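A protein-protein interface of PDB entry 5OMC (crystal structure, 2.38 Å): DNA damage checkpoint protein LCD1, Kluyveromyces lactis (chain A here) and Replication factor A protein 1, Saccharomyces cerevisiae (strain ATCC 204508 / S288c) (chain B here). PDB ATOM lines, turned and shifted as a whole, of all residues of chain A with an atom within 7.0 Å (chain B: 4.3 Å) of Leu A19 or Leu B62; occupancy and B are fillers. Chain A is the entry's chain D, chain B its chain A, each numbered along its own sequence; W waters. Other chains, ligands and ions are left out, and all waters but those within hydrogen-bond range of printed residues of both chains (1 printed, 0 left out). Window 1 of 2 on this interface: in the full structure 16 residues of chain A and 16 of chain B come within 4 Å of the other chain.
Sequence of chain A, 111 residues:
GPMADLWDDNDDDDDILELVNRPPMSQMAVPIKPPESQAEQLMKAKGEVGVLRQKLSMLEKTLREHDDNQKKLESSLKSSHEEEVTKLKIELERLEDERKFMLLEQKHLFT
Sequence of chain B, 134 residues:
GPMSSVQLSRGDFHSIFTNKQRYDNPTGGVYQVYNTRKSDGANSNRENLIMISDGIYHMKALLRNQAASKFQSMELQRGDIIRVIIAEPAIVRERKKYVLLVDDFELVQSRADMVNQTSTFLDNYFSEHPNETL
Along chain A the printed residues that touch a printed residue of chain B span positions 13 to 22. Among the printed residues, no Asp or Glu carboxylate lies within 4 Å of a Lys or Arg side-chain nitrogen of the other chain.
Printed residues of chain B within 4 Å of Asp A13: Leu B49 (3.5 Å). Of chain B, only Leu B62 (3.9 Å), Arg B64 (2.9 Å), Val B92 (3.9 Å), Val B99 (3.96 Å) and Leu B101 (3.8 Å) come within 4 Å of Leu A19. Ala B61 touches none of the printed residues of chain A. Of the printed residues of chain A, Leu B62 touches Ile A16, Leu A17, Leu A19 and Val A20. Leu B63 touches none of the printed residues of chain A. Printed residues of chain A within 4 Å of Val B92: Asp A15 (3.6 Å), Ile A16 (3.8 Å) and Leu A19 (3.9 Å). The nearest printed residue of chain B that does not touch Leu A19 is Ala B90 (4.3 Å).
NH1 of Arg B64 lies within hydrogen-bond range of O of Leu A19 (2.9 Å). NH1 of Arg B64 lies within hydrogen-bond range of O of Arg A22 (3.4 Å).
Water W1 lies within hydrogen-bond range of the guanidinium group (NE) of Arg A22, the backbone carbonyl oxygen (O) of Pro A23 and the guanidinium group (NH1) of Arg B64.
Among the printed residues, merely in contact across the chains: Arg A22 with Leu B101 (3.3 Å), Asp A13 with Leu B49 (3.5 Å), Ile A16 with Leu B62 (3.5 Å), Val A20 with Leu B62 (3.6 Å), Ile A16 with Val B99 (3.6 Å), Asp A15 with Val B92 (3.6 Å), Ile A16 with Leu B49 (3.7 Å), Val A20 with Arg B64 (3.7 Å), Ile A16 with Val B92 (3.8 Å), Leu A19 with Leu B101 (3.8 Å), Leu A19 with Val B92 (3.9 Å), Leu A19 with Leu B62 (3.9 Å), Leu A17 with Leu B62 (3.9 Å) and Leu A19 with Val B99 (3.96 Å).
The backbone NH of Leu B62 sits at hydrogen-bond distance from the backbone carbonyl oxygen of Leu B100, at 2.9 Å. The backbone carbonyl oxygen (O) of Leu B62 sits at hydrogen-bond distance from the backbone NH (N) of Val B102 (2.8 Å). The backbone carbonyl oxygen (O) of Val B102 lies within hydrogen-bond range of the backbone NH (N) of Arg B64 (2.8 Å). N of Ala B90 lies within hydrogen-bond range of O of Val B99 (3.0 Å).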
ATOM      1  N   ASP A  13     -30.665  21.519  30.908  1.00  0.00           N
ATOM      2  CA  ASP A  13     -29.979  22.347  29.906  1.00  0.00           C
ATOM      3  C   ASP A  13     -29.498  23.699  30.411  1.00  0.00           C
ATOM      4  O   ASP A  13     -29.443  24.667  29.658  1.00  0.00           O
ATOM      5  CB  ASP A  13     -30.840  22.532  28.646  1.00  0.00           C
ATOM      6  CG  ASP A  13     -31.184  21.253  27.919  1.00  0.00           C
ATOM      7  OD1 ASP A  13     -32.394  20.994  27.726  1.00  0.00           O
ATOM      8  OD2 ASP A  13     -30.241  20.505  27.540  1.00  0.00           O
ATOM      9  N   ASP A  14     -29.089  23.742  31.654  1.00  0.00           N
ATOM     10  CA  ASP A  14     -28.537  24.924  32.313  1.00  0.00           C
ATOM     11  C   ASP A  14     -27.225  25.423  31.644  1.00  0.00           C
ATOM     12  O   ASP A  14     -27.028  26.634  31.526  1.00  0.00           O
ATOM     13  CB  ASP A  14     -28.323  24.610  33.814  1.00  0.00           C
ATOM     14  CG  ASP A  14     -29.590  24.136  34.519  1.00  0.00           C
ATOM     15  OD1 ASP A  14     -30.599  24.879  34.473  1.00  0.00           O
ATOM     16  OD2 ASP A  14     -29.601  22.967  35.036  1.00  0.00           O
ATOM     17  N   ASP A  15     -26.360  24.480  31.177  1.00  0.00           N
ATOM     18  CA  ASP A  15     -25.090  24.762  30.482  1.00  0.00           C
ATOM     19  C   ASP A  15     -25.347  25.346  29.090  1.00  0.00           C
ATOM     20  O   ASP A  15     -24.458  25.979  28.524  1.00  0.00           O
ATOM     21  CB  ASP A  15     -24.163  23.517  30.407  1.00  0.00           C
ATOM     22  CG  ASP A  15     -24.823  22.192  30.043  1.00  0.00           C
ATOM     23  OD1 ASP A  15     -25.735  22.198  29.198  1.00  0.00           O
ATOM     24  OD2 ASP A  15     -24.422  21.149  30.617  1.00  0.00           O
ATOM     25  N   ILE A  16     -26.539  25.089  28.523  1.00  0.00           N
ATOM     26  CA  ILE A  16     -26.950  25.662  27.248  1.00  0.00           C
ATOM     27  C   ILE A  16     -27.486  27.079  27.495  1.00  0.00           C
ATOM     28  O   ILE A  16     -27.016  28.025  26.861  1.00  0.00           O
ATOM     29  CB  ILE A  16     -27.950  24.775  26.465  1.00  0.00           C
ATOM     30  CG1 ILE A  16     -27.306  23.394  26.076  1.00  0.00           C
ATOM     31  CG2 ILE A  16     -28.463  25.542  25.244  1.00  0.00           C
ATOM     32  CD1 ILE A  16     -28.240  22.416  25.326  1.00  0.00           C
ATOM     33  N   LEU A  17     -28.431  27.218  28.452  1.00  0.00           N
ATOM     34  CA  LEU A  17     -29.089  28.469  28.849  1.00  0.00           C
ATOM     35  C   LEU A  17     -28.115  29.547  29.322  1.00  0.00           C
ATOM     36  O   LEU A  17     -28.394  30.739  29.204  1.00  0.00           O
ATOM     37  CB  LEU A  17     -30.182  28.178  29.889  1.00  0.00           C
ATOM     38  CG  LEU A  17     -31.375  27.352  29.362  1.00  0.00           C
ATOM     39  CD1 LEU A  17     -32.071  26.602  30.489  1.00  0.00           C
ATOM     40  CD2 LEU A  17     -32.342  28.205  28.520  1.00  0.00           C
ATOM     41  N   GLU A  18     -26.932  29.128  29.746  1.00  0.00           N
ATOM     42  CA  GLU A  18     -25.859  29.989  30.220  1.00  0.00           C
ATOM     43  C   GLU A  18     -25.255  30.838  29.076  1.00  0.00           C
ATOM     44  O   GLU A  18     -24.596  31.840  29.343  1.00  0.00           O
ATOM     45  CB  GLU A  18     -24.789  29.059  30.803  1.00  0.00           C
ATOM     46  CG  GLU A  18     -23.888  29.586  31.892  1.00  0.00           C
ATOM     47  CD  GLU A  18     -22.512  28.944  31.759  1.00  0.00           C
ATOM     48  OE1 GLU A  18     -22.381  27.707  31.921  1.00  0.00           O
ATOM     49  OE2 GLU A  18     -21.576  29.678  31.368  1.00  0.00           O
ATOM     50  N   LEU A  19     -25.476  30.422  27.815  1.00  0.00           N
ATOM     51  CA  LEU A  19     -24.977  31.057  26.607  1.00  0.00           C
ATOM     52  C   LEU A  19     -25.834  32.214  26.128  1.00  0.00           C
ATOM     53  O   LEU A  19     -25.387  32.937  25.222  1.00  0.00           O
ATOM     54  CB  LEU A  19     -24.810  30.015  25.492  1.00  0.00           C
ATOM     55  CG  LEU A  19     -23.858  28.820  25.803  1.00  0.00           C
ATOM     56  CD1 LEU A  19     -24.178  27.630  24.927  1.00  0.00           C
ATOM     57  CD2 LEU A  19     -22.387  29.215  25.719  1.00  0.00           C
ATOM     58  N   VAL A  20     -27.042  32.413  26.730  1.00  0.00           N
ATOM     59  CA  VAL A  20     -28.000  33.505  26.410  1.00  0.00           C
ATOM     60  C   VAL A  20     -27.318  34.895  26.416  1.00  0.00           C
ATOM     61  O   VAL A  20     -27.576  35.737  25.540  1.00  0.00           O
ATOM     62  CB  VAL A  20     -29.267  33.499  27.335  1.00  0.00           C
ATOM     63  CG1 VAL A  20     -30.180  34.697  27.066  1.00  0.00           C
ATOM     64  CG2 VAL A  20     -30.061  32.204  27.190  1.00  0.00           C
ATOM     65  N   ASN A  21     -26.454  35.109  27.417  1.00  0.00           N
ATOM     66  CA  ASN A  21     -25.762  36.367  27.677  1.00  0.00           C
ATOM     67  C   ASN A  21     -24.315  36.408  27.230  1.00  0.00           C
ATOM     68  O   ASN A  21     -23.663  37.437  27.437  1.00  0.00           O
ATOM     69  CB  ASN A  21     -25.872  36.713  29.164  1.00  0.00           C
ATOM     70  CG  ASN A  21     -27.297  36.906  29.596  1.00  0.00           C
ATOM     71  OD1 ASN A  21     -28.008  37.812  29.125  1.00  0.00           O
ATOM     72  ND2 ASN A  21     -27.757  35.999  30.446  1.00  0.00           N
ATOM     73  N   ARG A  22     -23.810  35.310  26.617  1.00  0.00           N
ATOM     74  CA  ARG A  22     -22.446  35.255  26.102  1.00  0.00           C
ATOM     75  C   ARG A  22     -22.364  36.273  24.988  1.00  0.00           C
ATOM     76  O   ARG A  22     -23.261  36.305  24.143  1.00  0.00           O
ATOM     77  CB  ARG A  22     -22.084  33.861  25.574  1.00  0.00           C
ATOM     78  CG  ARG A  22     -20.579  33.669  25.416  1.00  0.00           C
ATOM     79  CD  ARG A  22     -20.198  32.293  24.947  1.00  0.00           C
ATOM     80  NE  ARG A  22     -20.592  32.079  23.561  1.00  0.00           N
ATOM     81  CZ  ARG A  22     -20.316  30.983  22.865  1.00  0.00           C
ATOM     82  NH1 ARG A  22     -19.617  29.994  23.417  1.00  0.00           N
ATOM     83  NH2 ARG A  22     -20.724  30.869  21.608  1.00  0.00           N
ATOM     84  N   PRO A  23     -21.368  37.187  25.022  1.00  0.00           N
ATOM     85  CA  PRO A  23     -21.304  38.223  23.972  1.00  0.00           C
ATOM     86  C   PRO A  23     -21.325  37.627  22.558  1.00  0.00           C
ATOM     87  O   PRO A  23     -20.586  36.670  22.275  1.00  0.00           O
ATOM     88  CB  PRO A  23     -20.008  38.983  24.271  1.00  0.00           C
ATOM     89  CG  PRO A  23     -19.342  38.232  25.303  1.00  0.00           C
ATOM     90  CD  PRO A  23     -20.266  37.325  25.993  1.00  0.00           C
ATOM     91  N   ASN B  48     -36.892  30.057  25.393  1.00  0.00           N
ATOM     92  CA  ASN B  48     -36.019  30.427  24.284  1.00  0.00           C
ATOM     93  C   ASN B  48     -35.186  29.255  23.778  1.00  0.00           C
ATOM     94  O   ASN B  48     -34.551  29.355  22.728  1.00  0.00           O
ATOM     95  CB  ASN B  48     -35.164  31.631  24.652  1.00  0.00           C
ATOM     96  CG  ASN B  48     -35.978  32.898  24.806  1.00  0.00           C
ATOM     97  OD1 ASN B  48     -37.057  33.077  24.206  1.00  0.00           O
ATOM     98  ND2 ASN B  48     -35.468  33.809  25.614  1.00  0.00           N
ATOM     99  N   LEU B  49     -35.234  28.128  24.496  1.00  0.00           N
ATOM    100  CA  LEU B  49     -34.563  26.903  24.099  1.00  0.00           C
ATOM    101  C   LEU B  49     -35.623  26.035  23.437  1.00  0.00           C
ATOM    102  O   LEU B  49     -36.609  25.663  24.069  1.00  0.00           O
ATOM    103  CB  LEU B  49     -33.892  26.202  25.301  1.00  0.00           C
ATOM    104  CG  LEU B  49     -32.965  25.021  24.979  1.00  0.00           C
ATOM    105  CD1 LEU B  49     -31.937  25.378  23.896  1.00  0.00           C
ATOM    106  CD2 LEU B  49     -32.278  24.546  26.213  1.00  0.00           C
ATOM    107  N   ALA B  61     -31.951  24.594  19.711  1.00  0.00           N
ATOM    108  CA  ALA B  61     -31.640  25.949  19.277  1.00  0.00           C
ATOM    109  C   ALA B  61     -31.902  26.880  20.442  1.00  0.00           C
ATOM    110  O   ALA B  61     -32.958  26.810  21.064  1.00  0.00           O
ATOM    111  CB  ALA B  61     -32.522  26.343  18.088  1.00  0.00           C
ATOM    112  N   LEU B  62     -30.927  27.718  20.763  1.00  0.00           N
ATOM    113  CA  LEU B  62     -31.101  28.711  21.807  1.00  0.00           C
ATOM    114  C   LEU B  62     -31.293  30.060  21.117  1.00  0.00           C
ATOM    115  O   LEU B  62     -30.395  30.538  20.401  1.00  0.00           O
ATOM    116  CB  LEU B  62     -29.936  28.750  22.813  1.00  0.00           C
ATOM    117  CG  LEU B  62     -30.048  29.832  23.919  1.00  0.00           C
ATOM    118  CD1 LEU B  62     -31.157  29.479  24.975  1.00  0.00           C
ATOM    119  CD2 LEU B  62     -28.678  30.104  24.540  1.00  0.00           C
ATOM    120  N   LEU B  63     -32.490  30.641  21.279  1.00  0.00           N
ATOM    121  CA  LEU B  63     -32.818  31.936  20.692  1.00  0.00           C
ATOM    122  C   LEU B  63     -32.293  33.021  21.587  1.00  0.00           C
ATOM    123  O   LEU B  63     -32.491  32.976  22.802  1.00  0.00           O
ATOM    124  CB  LEU B  63     -34.324  32.107  20.518  1.00  0.00           C
ATOM    125  CG  LEU B  63     -35.025  31.089  19.596  1.00  0.00           C
ATOM    126  CD1 LEU B  63     -36.457  30.845  20.064  1.00  0.00           C
ATOM    127  CD2 LEU B  63     -34.982  31.522  18.146  1.00  0.00           C
ATOM    128  N   ARG B  64     -31.561  33.981  21.007  1.00  0.00           N
ATOM    129  CA  ARG B  64     -31.012  35.100  21.770  1.00  0.00           C
ATOM    130  C   ARG B  64     -31.307  36.375  21.033  1.00  0.00           C
ATOM    131  O   ARG B  64     -31.780  36.342  19.893  1.00  0.00           O
ATOM    132  CB  ARG B  64     -29.487  34.959  21.969  1.00  0.00           C
ATOM    133  CG  ARG B  64     -28.988  33.558  22.241  1.00  0.00           C
ATOM    134  CD  ARG B  64     -27.520  33.523  22.528  1.00  0.00           C
ATOM    135  NE  ARG B  64     -26.741  34.025  21.401  1.00  0.00           N
ATOM    136  CZ  ARG B  64     -25.425  34.164  21.425  1.00  0.00           C
ATOM    137  NH1 ARG B  64     -24.734  33.789  22.486  1.00  0.00           N
ATOM    138  NH2 ARG B  64     -24.788  34.655  20.377  1.00  0.00           N
ATOM    139  N   ALA B  90     -22.328  25.888  18.834  1.00  0.00           N
ATOM    140  CA  ALA B  90     -21.774  25.722  20.178  1.00  0.00           C
ATOM    141  C   ALA B  90     -21.913  24.285  20.655  1.00  0.00           C
ATOM    142  O   ALA B  90     -22.948  23.658  20.424  1.00  0.00           O
ATOM    143  CB  ALA B  90     -22.416  26.700  21.159  1.00  0.00           C
ATOM    144  N   VAL B  92     -21.372  21.969  24.163  1.00  0.00           N
ATOM    145  CA  VAL B  92     -21.212  22.061  25.623  1.00  0.00           C
ATOM    146  C   VAL B  92     -21.142  20.677  26.275  1.00  0.00           C
ATOM    147  O   VAL B  92     -21.179  19.661  25.573  1.00  0.00           O
ATOM    148  CB  VAL B  92     -22.269  22.993  26.307  1.00  0.00           C
ATOM    149  CG1 VAL B  92     -22.225  24.414  25.750  1.00  0.00           C
ATOM    150  CG2 VAL B  92     -23.671  22.420  26.216  1.00  0.00           C
ATOM    151  N   VAL B  99     -25.794  22.731  20.352  1.00  0.00           N
ATOM    152  CA  VAL B  99     -26.747  23.843  20.291  1.00  0.00           C
ATOM    153  C   VAL B  99     -26.392  24.857  19.203  1.00  0.00           C
ATOM    154  O   VAL B  99     -25.220  25.176  18.987  1.00  0.00           O
ATOM    155  CB  VAL B  99     -26.957  24.527  21.670  1.00  0.00           C
ATOM    156  CG1 VAL B  99     -25.690  25.253  22.147  1.00  0.00           C
ATOM    157  CG2 VAL B  99     -28.163  25.468  21.643  1.00  0.00           C
ATOM    158  N   LEU B 100     -27.412  25.358  18.524  1.00  0.00           N
ATOM    159  CA  LEU B 100     -27.269  26.423  17.537  1.00  0.00           C
ATOM    160  C   LEU B 100     -27.786  27.671  18.219  1.00  0.00           C
ATOM    161  O   LEU B 100     -28.967  27.730  18.592  1.00  0.00           O
ATOM    162  CB  LEU B 100     -28.070  26.140  16.245  1.00  0.00           C
ATOM    163  CG  LEU B 100     -27.890  27.155  15.105  1.00  0.00           C
ATOM    164  CD1 LEU B 100     -26.492  27.049  14.468  1.00  0.00           C
ATOM    165  CD2 LEU B 100     -28.949  26.974  14.065  1.00  0.00           C
ATOM    166  N   LEU B 101     -26.893  28.645  18.443  1.00  0.00           N
ATOM    167  CA  LEU B 101     -27.294  29.910  19.067  1.00  0.00           C
ATOM    168  C   LEU B 101     -27.837  30.804  17.943  1.00  0.00           C
ATOM    169  O   LEU B 101     -27.079  31.206  17.060  1.00  0.00           O
ATOM    170  CB  LEU B 101     -26.118  30.586  19.819  1.00  0.00           C
ATOM    171  CG  LEU B 101     -25.233  29.667  20.681  1.00  0.00           C
ATOM    172  CD1 LEU B 101     -23.939  30.340  21.006  1.00  0.00           C
ATOM    173  CD2 LEU B 101     -25.964  29.214  21.968  1.00  0.00           C
ATOM    174  N   VAL B 102     -29.161  31.048  17.950  1.00  0.00           N
ATOM    175  CA  VAL B 102     -29.830  31.840  16.904  1.00  0.00           C
ATOM    176  C   VAL B 102     -30.103  33.252  17.408  1.00  0.00           C
ATOM    177  O   VAL B 102     -30.830  33.417  18.381  1.00  0.00           O
ATOM    178  CB  VAL B 102     -31.087  31.111  16.328  1.00  0.00           C
ATOM    179  CG1 VAL B 102     -31.789  31.947  15.261  1.00  0.00           C
ATOM    180  CG2 VAL B 102     -30.709  29.756  15.765  1.00  0.00           C
HETATM  181  O   HOH W   1     -21.613  33.968  21.786  1.00  0.00           O
